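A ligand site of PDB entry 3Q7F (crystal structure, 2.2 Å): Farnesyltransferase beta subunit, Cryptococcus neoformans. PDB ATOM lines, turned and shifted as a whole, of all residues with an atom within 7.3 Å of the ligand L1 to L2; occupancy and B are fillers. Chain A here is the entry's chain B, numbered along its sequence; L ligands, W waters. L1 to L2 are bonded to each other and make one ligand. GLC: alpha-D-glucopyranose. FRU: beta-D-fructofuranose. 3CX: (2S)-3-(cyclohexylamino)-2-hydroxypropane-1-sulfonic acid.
CG2 of Thr 3 touches O6 of GLC L1 (3.7 Å). Pro 47 touches the ligand L1 to L2. O of Glu 484 touches O4 of FRU L2, 3.9 Å away. C of Ile 485 touches O4 of FRU L2 (3.6 Å). Val 487 touches the ligand L1 to L2. CA of Gly 489 touches O3 of FRU L2 (3.8 Å). CE of Lys 490 touches O1 of FRU L2, 3.6 Å away. Hydrophobic or aromatic side chains within 4 Å of the ligand L1 to L2: Ile 486. The nearest printed residue that does not touch the ligand L1 to L2 is Ala 49 (4.7 Å).
The backbone NH (N) of Ile 486 sits at hydrogen-bond distance from an oxygen (O4) of FRU L2, 2.6 Å away. The backbone carbonyl oxygen of Ile 486 is in hydrogen-bond range of an oxygen (O3) of FRU L2 (2.8 Å). O4 of GLC L1 is in hydrogen-bond range of N of Gly 488. O of Asn 48 sits at hydrogen-bond distance from O3 of GLC L1 (3.2 Å). O4 of GLC L1 lies within hydrogen-bond range of OD1 of Asn 48 (2.9 Å). An oxygen (OAD) of 3CX L3 sits at hydrogen-bond distance from the backbone NH (N) of Lys 490, 2.9 Å away. An oxygen (OAC) of 3CX L3 is in hydrogen-bond range of the backbone NH (N) of Asp 491 (3.4 Å). NAL of 3CX L3 is in salt-bridge range of OD2 of Asp 491 (2.5 Å).
Water W1 lies within hydrogen-bond range of O6 of GLC L1 (2.6 Å) and OD1 of Asn 48 (2.7 Å). Water W3 lies within hydrogen-bond range of an oxygen (O3) of GLC L1 (2.7 Å) and the backbone carbonyl oxygen (O) of Gly 488 (3.2 Å). Water W2 bridges OAD of 3CX L3 (2.8 Å) and O2 of GLC L1 (3.0 Å). Water W5 lies within hydrogen-bond range of OE2 of Glu 484 and O4 of FRU L2.
The backbone NH of Asn 48 sits at hydrogen-bond distance from the side-chain carboxylate of Asp 46, at 2.9 Å. ND2 of Asn 48 sits at hydrogen-bond distance from OE2 of Glu 382. N of Val 487 sits close to NE2 of Gln 381. ND2 of Asn 492 lies within hydrogen-bond range of O of Val 487 (2.8 Å). The backbone carbonyl oxygen of Gln 422 lies within hydrogen-bond range of the backbone NH of Ile 485 (2.9 Å). The backbone carbonyl oxygen (O) of Ile 485 lies close to the side-chain amide oxygen (OE1) of Gln 381, at 2.8 Å. O of Thr 3 lies close to OG1 of Thr 6 (3.4 Å). The side-chain carboxylate of Glu 484 lies within salt-bridge range of the guanidinium group of Arg 493.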
ATOM      1  N   ALA A   2     -28.685   2.700 -26.267  1.00  0.00           N
ATOM      2  CA  ALA A   2     -29.470   3.774 -26.948  1.00  0.00           C
ATOM      3  C   ALA A   2     -28.647   4.527 -28.003  1.00  0.00           C
ATOM      4  O   ALA A   2     -29.197   4.979 -29.021  1.00  0.00           O
ATOM      5  CB  ALA A   2     -30.039   4.750 -25.926  1.00  0.00           C
ATOM      6  N   THR A   3     -27.339   4.646 -27.757  1.00  0.00           N
ATOM      7  CA  THR A   3     -26.443   5.410 -28.626  1.00  0.00           C
ATOM      8  C   THR A   3     -25.488   4.539 -29.451  1.00  0.00           C
ATOM      9  O   THR A   3     -24.565   5.051 -30.093  1.00  0.00           O
ATOM     10  CB  THR A   3     -25.631   6.454 -27.834  1.00  0.00           C
ATOM     11  OG1 THR A   3     -24.762   5.773 -26.913  1.00  0.00           O
ATOM     12  CG2 THR A   3     -26.547   7.401 -27.065  1.00  0.00           C
ATOM     13  N   THR A   6     -25.579   5.555 -33.034  1.00  0.00           N
ATOM     14  CA  THR A   6     -25.524   7.004 -33.212  1.00  0.00           C
ATOM     15  C   THR A   6     -24.206   7.561 -32.661  1.00  0.00           C
ATOM     16  O   THR A   6     -24.196   8.182 -31.591  1.00  0.00           O
ATOM     17  CB  THR A   6     -26.719   7.724 -32.534  1.00  0.00           C
ATOM     18  OG1 THR A   6     -26.763   7.392 -31.143  1.00  0.00           O
ATOM     19  CG2 THR A   6     -28.036   7.327 -33.190  1.00  0.00           C
ATOM     20  N   ASP A  46     -16.164  18.579 -25.986  1.00  0.00           N
ATOM     21  CA  ASP A  46     -17.082  17.492 -26.317  1.00  0.00           C
ATOM     22  C   ASP A  46     -18.245  17.489 -25.324  1.00  0.00           C
ATOM     23  O   ASP A  46     -18.030  17.301 -24.129  1.00  0.00           O
ATOM     24  CB  ASP A  46     -16.301  16.171 -26.279  1.00  0.00           C
ATOM     25  CG  ASP A  46     -17.152  14.948 -26.640  1.00  0.00           C
ATOM     26  OD1 ASP A  46     -18.380  15.041 -26.810  1.00  0.00           O
ATOM     27  OD2 ASP A  46     -16.555  13.856 -26.737  1.00  0.00           O
ATOM     28  N   PRO A  47     -19.488  17.698 -25.808  1.00  0.00           N
ATOM     29  CA  PRO A  47     -20.675  17.729 -24.935  1.00  0.00           C
ATOM     30  C   PRO A  47     -20.864  16.444 -24.121  1.00  0.00           C
ATOM     31  O   PRO A  47     -21.429  16.487 -23.035  1.00  0.00           O
ATOM     32  CB  PRO A  47     -21.838  17.892 -25.905  1.00  0.00           C
ATOM     33  CG  PRO A  47     -21.252  18.413 -27.154  1.00  0.00           C
ATOM     34  CD  PRO A  47     -19.853  17.895 -27.222  1.00  0.00           C
ATOM     35  N   ASN A  48     -20.376  15.320 -24.659  1.00  0.00           N
ATOM     36  CA  ASN A  48     -20.540  14.007 -24.036  1.00  0.00           C
ATOM     37  C   ASN A  48     -19.589  13.720 -22.875  1.00  0.00           C
ATOM     38  O   ASN A  48     -19.832  12.811 -22.080  1.00  0.00           O
ATOM     39  CB  ASN A  48     -20.423  12.904 -25.089  1.00  0.00           C
ATOM     40  CG  ASN A  48     -21.400  13.088 -26.245  1.00  0.00           C
ATOM     41  OD1 ASN A  48     -22.583  12.770 -26.122  1.00  0.00           O
ATOM     42  ND2 ASN A  48     -20.896  13.587 -27.366  1.00  0.00           N
ATOM     43  N   ALA A  49     -18.497  14.482 -22.786  1.00  0.00           N
ATOM     44  CA  ALA A  49     -17.438  14.223 -21.804  1.00  0.00           C
ATOM     45  C   ALA A  49     -17.835  14.570 -20.371  1.00  0.00           C
ATOM     46  O   ALA A  49     -18.586  15.518 -20.127  1.00  0.00           O
ATOM     47  CB  ALA A  49     -16.160  14.963 -22.201  1.00  0.00           C
ATOM     48  N   LEU A  50     -17.322  13.790 -19.419  1.00  0.00           N
ATOM     49  CA  LEU A  50     -17.474  14.099 -17.993  1.00  0.00           C
ATOM     50  C   LEU A  50     -16.487  15.184 -17.587  1.00  0.00           C
ATOM     51  O   LEU A  50     -16.890  16.234 -17.073  1.00  0.00           O
ATOM     52  CB  LEU A  50     -17.264  12.845 -17.121  1.00  0.00           C
ATOM     53  CG  LEU A  50     -18.478  11.968 -16.784  1.00  0.00           C
ATOM     54  CD1 LEU A  50     -18.029  10.723 -16.021  1.00  0.00           C
ATOM     55  CD2 LEU A  50     -19.540  12.742 -15.998  1.00  0.00           C
ATOM     56  N   VAL A 378     -27.475  11.849 -32.255  1.00  0.00           N
ATOM     57  CA  VAL A 378     -26.444  12.459 -31.413  1.00  0.00           C
ATOM     58  C   VAL A 378     -25.670  13.538 -32.185  1.00  0.00           C
ATOM     59  O   VAL A 378     -25.505  14.663 -31.687  1.00  0.00           O
ATOM     60  CB  VAL A 378     -25.485  11.386 -30.816  1.00  0.00           C
ATOM     61  CG1 VAL A 378     -24.249  12.019 -30.201  1.00  0.00           C
ATOM     62  CG2 VAL A 378     -26.220  10.535 -29.795  1.00  0.00           C
ATOM     63  N   GLN A 381     -27.610  16.789 -32.686  1.00  0.00           N
ATOM     64  CA  GLN A 381     -27.612  17.592 -31.461  1.00  0.00           C
ATOM     65  C   GLN A 381     -26.275  18.315 -31.279  1.00  0.00           C
ATOM     66  O   GLN A 381     -26.261  19.483 -30.891  1.00  0.00           O
ATOM     67  CB  GLN A 381     -27.931  16.734 -30.240  1.00  0.00           C
ATOM     68  CG  GLN A 381     -29.345  16.186 -30.242  1.00  0.00           C
ATOM     69  CD  GLN A 381     -29.667  15.386 -29.014  1.00  0.00           C
ATOM     70  OE1 GLN A 381     -30.029  14.216 -29.114  1.00  0.00           O
ATOM     71  NE2 GLN A 381     -29.536  16.003 -27.852  1.00  0.00           N
ATOM     72  N   GLU A 382     -25.179  17.617 -31.579  1.00  0.00           N
ATOM     73  CA  GLU A 382     -23.847  18.205 -31.522  1.00  0.00           C
ATOM     74  C   GLU A 382     -23.672  19.361 -32.511  1.00  0.00           C
ATOM     75  O   GLU A 382     -23.083  20.379 -32.163  1.00  0.00           O
ATOM     76  CB  GLU A 382     -22.769  17.141 -31.727  1.00  0.00           C
ATOM     77  CG  GLU A 382     -22.651  16.171 -30.567  1.00  0.00           C
ATOM     78  CD  GLU A 382     -21.720  15.007 -30.857  1.00  0.00           C
ATOM     79  OE1 GLU A 382     -21.661  14.570 -32.030  1.00  0.00           O
ATOM     80  OE2 GLU A 382     -21.059  14.524 -29.917  1.00  0.00           O
ATOM     81  N   GLN A 422     -33.710  14.941 -30.061  1.00  0.00           N
ATOM     82  CA  GLN A 422     -33.753  14.669 -28.622  1.00  0.00           C
ATOM     83  C   GLN A 422     -34.794  13.619 -28.243  1.00  0.00           C
ATOM     84  O   GLN A 422     -34.528  12.756 -27.409  1.00  0.00           O
ATOM     85  CB  GLN A 422     -34.006  15.950 -27.827  1.00  0.00           C
ATOM     86  CG  GLN A 422     -32.757  16.806 -27.603  1.00  0.00           C
ATOM     87  CD  GLN A 422     -32.998  17.984 -26.664  1.00  0.00           C
ATOM     88  OE1 GLN A 422     -34.121  18.199 -26.184  1.00  0.00           O
ATOM     89  NE2 GLN A 422     -31.951  18.749 -26.401  1.00  0.00           N
ATOM     90  N   GLY A 482     -38.349   5.528 -23.036  1.00  0.00           N
ATOM     91  CA  GLY A 482     -36.958   5.103 -23.148  1.00  0.00           C
ATOM     92  C   GLY A 482     -36.238   5.607 -24.386  1.00  0.00           C
ATOM     93  O   GLY A 482     -35.062   5.302 -24.596  1.00  0.00           O
ATOM     94  N   GLU A 484     -35.604   8.788 -25.234  1.00  0.00           N
ATOM     95  CA  GLU A 484     -34.994  10.103 -25.058  1.00  0.00           C
ATOM     96  C   GLU A 484     -33.468  10.048 -25.053  1.00  0.00           C
ATOM     97  O   GLU A 484     -32.866   9.225 -24.357  1.00  0.00           O
ATOM     98  CB  GLU A 484     -35.495  10.756 -23.768  1.00  0.00           C
ATOM     99  CG  GLU A 484     -35.285  12.247 -23.699  1.00  0.00           C
ATOM    100  CD  GLU A 484     -35.763  12.868 -22.400  1.00  0.00           C
ATOM    101  OE1 GLU A 484     -36.543  13.850 -22.456  1.00  0.00           O
ATOM    102  OE2 GLU A 484     -35.375  12.377 -21.318  1.00  0.00           O
ATOM    103  N   ILE A 485     -32.847  10.901 -25.865  1.00  0.00           N
ATOM    104  CA  ILE A 485     -31.401  11.106 -25.833  1.00  0.00           C
ATOM    105  C   ILE A 485     -31.111  12.603 -25.780  1.00  0.00           C
ATOM    106  O   ILE A 485     -31.296  13.306 -26.775  1.00  0.00           O
ATOM    107  CB  ILE A 485     -30.657  10.448 -27.041  1.00  0.00           C
ATOM    108  CG1 ILE A 485     -30.972   8.946 -27.142  1.00  0.00           C
ATOM    109  CG2 ILE A 485     -29.148  10.647 -26.923  1.00  0.00           C
ATOM    110  CD1 ILE A 485     -30.529   8.302 -28.457  1.00  0.00           C
ATOM    111  N   ILE A 486     -30.669  13.070 -24.626  1.00  0.00           N
ATOM    112  CA  ILE A 486     -30.310  14.468 -24.444  1.00  0.00           C
ATOM    113  C   ILE A 486     -28.789  14.614 -24.326  1.00  0.00           C
ATOM    114  O   ILE A 486     -28.206  14.403 -23.259  1.00  0.00           O
ATOM    115  CB  ILE A 486     -31.002  15.124 -23.211  1.00  0.00           C
ATOM    116  CG1 ILE A 486     -32.474  14.693 -23.101  1.00  0.00           C
ATOM    117  CG2 ILE A 486     -30.851  16.649 -23.248  1.00  0.00           C
ATOM    118  CD1 ILE A 486     -33.392  15.208 -24.204  1.00  0.00           C
ATOM    119  N   VAL A 487     -28.172  14.948 -25.450  1.00  0.00           N
ATOM    120  CA  VAL A 487     -26.724  15.132 -25.548  1.00  0.00           C
ATOM    121  C   VAL A 487     -26.285  16.305 -24.671  1.00  0.00           C
ATOM    122  O   VAL A 487     -26.844  17.403 -24.758  1.00  0.00           O
ATOM    123  CB  VAL A 487     -26.290  15.345 -27.014  1.00  0.00           C
ATOM    124  CG1 VAL A 487     -24.824  15.785 -27.113  1.00  0.00           C
ATOM    125  CG2 VAL A 487     -26.525  14.080 -27.833  1.00  0.00           C
ATOM    126  N   GLY A 488     -25.297  16.061 -23.805  1.00  0.00           N
ATOM    127  CA  GLY A 488     -24.741  17.097 -22.942  1.00  0.00           C
ATOM    128  C   GLY A 488     -25.418  17.203 -21.579  1.00  0.00           C
ATOM    129  O   GLY A 488     -25.025  18.030 -20.747  1.00  0.00           O
ATOM    130  N   GLY A 489     -26.426  16.384 -21.341  1.00  0.00           N
ATOM    131  CA  GLY A 489     -27.116  16.374 -20.053  1.00  0.00           C
ATOM    132  C   GLY A 489     -28.484  17.024 -20.102  1.00  0.00           C
ATOM    133  O   GLY A 489     -28.810  17.726 -21.066  1.00  0.00           O
ATOM    134  N   LYS A 490     -29.270  16.818 -19.050  1.00  0.00           N
ATOM    135  CA  LYS A 490     -30.687  17.178 -19.034  1.00  0.00           C
ATOM    136  C   LYS A 490     -31.004  18.673 -19.085  1.00  0.00           C
ATOM    137  O   LYS A 490     -32.106  19.050 -19.455  1.00  0.00           O
ATOM    138  CB  LYS A 490     -31.403  16.497 -17.870  1.00  0.00           C
ATOM    139  CG  LYS A 490     -31.443  14.979 -18.013  1.00  0.00           C
ATOM    140  CD  LYS A 490     -32.157  14.311 -16.859  1.00  0.00           C
ATOM    141  CE  LYS A 490     -32.168  12.801 -17.024  1.00  0.00           C
ATOM    142  NZ  LYS A 490     -32.943  12.141 -15.936  1.00  0.00           N
ATOM    143  N   ASP A 491     -30.044  19.509 -18.728  1.00  0.00           N
ATOM    144  CA  ASP A 491     -30.222  20.967 -18.858  1.00  0.00           C
ATOM    145  C   ASP A 491     -30.328  21.416 -20.321  1.00  0.00           C
ATOM    146  O   ASP A 491     -30.845  22.497 -20.602  1.00  0.00           O
ATOM    147  CB  ASP A 491     -29.108  21.721 -18.138  1.00  0.00           C
ATOM    148  CG  ASP A 491     -29.237  21.656 -16.620  1.00  0.00           C
ATOM    149  OD1 ASP A 491     -30.352  21.851 -16.080  1.00  0.00           O
ATOM    150  OD2 ASP A 491     -28.214  21.438 -15.958  1.00  0.00           O
ATOM    151  N   ASN A 492     -29.848  20.584 -21.241  1.00  0.00           N
ATOM    152  CA  ASN A 492     -30.016  20.844 -22.683  1.00  0.00           C
ATOM    153  C   ASN A 492     -31.387  20.468 -23.246  1.00  0.00           C
ATOM    154  O   ASN A 492     -31.700  20.806 -24.388  1.00  0.00           O
ATOM    155  CB  ASN A 492     -28.937  20.131 -23.493  1.00  0.00           C
ATOM    156  CG  ASN A 492     -27.582  20.769 -23.339  1.00  0.00           C
ATOM    157  OD1 ASN A 492     -27.453  21.919 -22.910  1.00  0.00           O
ATOM    158  ND2 ASN A 492     -26.542  20.021 -23.693  1.00  0.00           N
ATOM    159  N   ARG A 493     -32.209  19.781 -22.445  1.00  0.00           N
ATOM    160  CA  ARG A 493     -33.530  19.316 -22.888  1.00  0.00           C
ATOM    161  C   ARG A 493     -34.475  20.456 -23.238  1.00  0.00           C
ATOM    162  O   ARG A 493     -34.688  21.377 -22.452  1.00  0.00           O
ATOM    163  CB  ARG A 493     -34.189  18.432 -21.821  1.00  0.00           C
ATOM    164  CG  ARG A 493     -35.526  17.812 -22.268  1.00  0.00           C
ATOM    165  CD  ARG A 493     -36.408  17.428 -21.082  1.00  0.00           C
ATOM    166  NE  ARG A 493     -37.669  16.823 -21.524  1.00  0.00           N
ATOM    167  CZ  ARG A 493     -38.773  17.513 -21.826  1.00  0.00           C
ATOM    168  NH1 ARG A 493     -38.801  18.840 -21.731  1.00  0.00           N
ATOM    169  NH2 ARG A 493     -39.872  16.873 -22.219  1.00  0.00           N
HETATM  170  C1  GLC L   1     -25.890  11.404 -20.839  1.00  0.00           C
HETATM  171  C2  GLC L   1     -24.775  12.410 -20.671  1.00  0.00           C
HETATM  172  C3  GLC L   1     -23.696  12.333 -21.725  1.00  0.00           C
HETATM  173  C4  GLC L   1     -24.232  12.230 -23.125  1.00  0.00           C
HETATM  174  C5  GLC L   1     -25.632  11.667 -23.097  1.00  0.00           C
HETATM  175  C6  GLC L   1     -26.002  11.070 -24.411  1.00  0.00           C
HETATM  176  O2  GLC L   1     -24.229  12.244 -19.432  1.00  0.00           O
HETATM  177  O3  GLC L   1     -22.881  13.437 -21.567  1.00  0.00           O
HETATM  178  O4  GLC L   1     -24.181  13.430 -23.835  1.00  0.00           O
HETATM  179  O5  GLC L   1     -25.835  10.734 -22.073  1.00  0.00           O
HETATM  180  O6  GLC L   1     -25.212   9.968 -24.723  1.00  0.00           O
HETATM  181  C1  FRU L   2     -27.818  11.653 -18.461  1.00  0.00           C
HETATM  182  C2  FRU L   2     -28.111  11.475 -19.908  1.00  0.00           C
HETATM  183  C3  FRU L   2     -29.411  12.117 -20.303  1.00  0.00           C
HETATM  184  C4  FRU L   2     -30.095  11.139 -21.188  1.00  0.00           C
HETATM  185  C5  FRU L   2     -29.098  10.055 -21.365  1.00  0.00           C
HETATM  186  C6  FRU L   2     -29.723   8.706 -21.559  1.00  0.00           C
HETATM  187  O1  FRU L   2     -28.919  11.368 -17.674  1.00  0.00           O
HETATM  188  O2  FRU L   2     -27.104  12.108 -20.691  1.00  0.00           O
HETATM  189  O3  FRU L   2     -29.220  13.362 -20.885  1.00  0.00           O
HETATM  190  O4  FRU L   2     -30.464  11.670 -22.403  1.00  0.00           O
HETATM  191  O5  FRU L   2     -28.235  10.120 -20.240  1.00  0.00           O
HETATM  192  O6  FRU L   2     -29.093   8.126 -22.650  1.00  0.00           O
HETATM  193  OAA 3CX L   3     -27.525  14.271 -14.866  1.00  0.00           O
HETATM  194  OAB 3CX L   3     -29.252  15.870 -15.253  1.00  0.00           O
HETATM  195  OAC 3CX L   3     -28.072  18.493 -16.183  1.00  0.00           O
HETATM  196  OAD 3CX L   3     -27.833  15.188 -17.064  1.00  0.00           O
HETATM  197  CAE 3CX L   3     -23.960  23.926 -15.153  1.00  0.00           C
HETATM  198  CAF 3CX L   3     -23.911  22.779 -14.191  1.00  0.00           C
HETATM  199  CAG 3CX L   3     -23.864  23.470 -16.579  1.00  0.00           C
HETATM  200  CAH 3CX L   3     -24.904  21.713 -14.517  1.00  0.00           C
HETATM  201  CAI 3CX L   3     -24.871  22.406 -16.914  1.00  0.00           C
HETATM  202  CAJ 3CX L   3     -25.807  19.073 -15.756  1.00  0.00           C
HETATM  203  CAK 3CX L   3     -26.762  16.769 -15.237  1.00  0.00           C
HETATM  204  NAL 3CX L   3     -25.985  20.403 -16.273  1.00  0.00           N
HETATM  205  CAM 3CX L   3     -26.958  18.113 -15.843  1.00  0.00           C
HETATM  206  CAN 3CX L   3     -24.851  21.263 -15.950  1.00  0.00           C
HETATM  207  SAO 3CX L   3     -27.895  15.474 -15.624  1.00  0.00           S
HETATM  208  O   HOH W   1     -23.666  10.386 -26.814  1.00  0.00           O
HETATM  209  O   HOH W   2     -25.169  14.618 -17.861  1.00  0.00           O
HETATM  210  O   HOH W   3     -23.193  15.526 -19.953  1.00  0.00           O
HETATM  211  O   HOH W   4     -33.202   8.404 -21.731  1.00  0.00           O
HETATM  212  O   HOH W   5     -32.941  12.128 -20.292  1.00  0.00           O
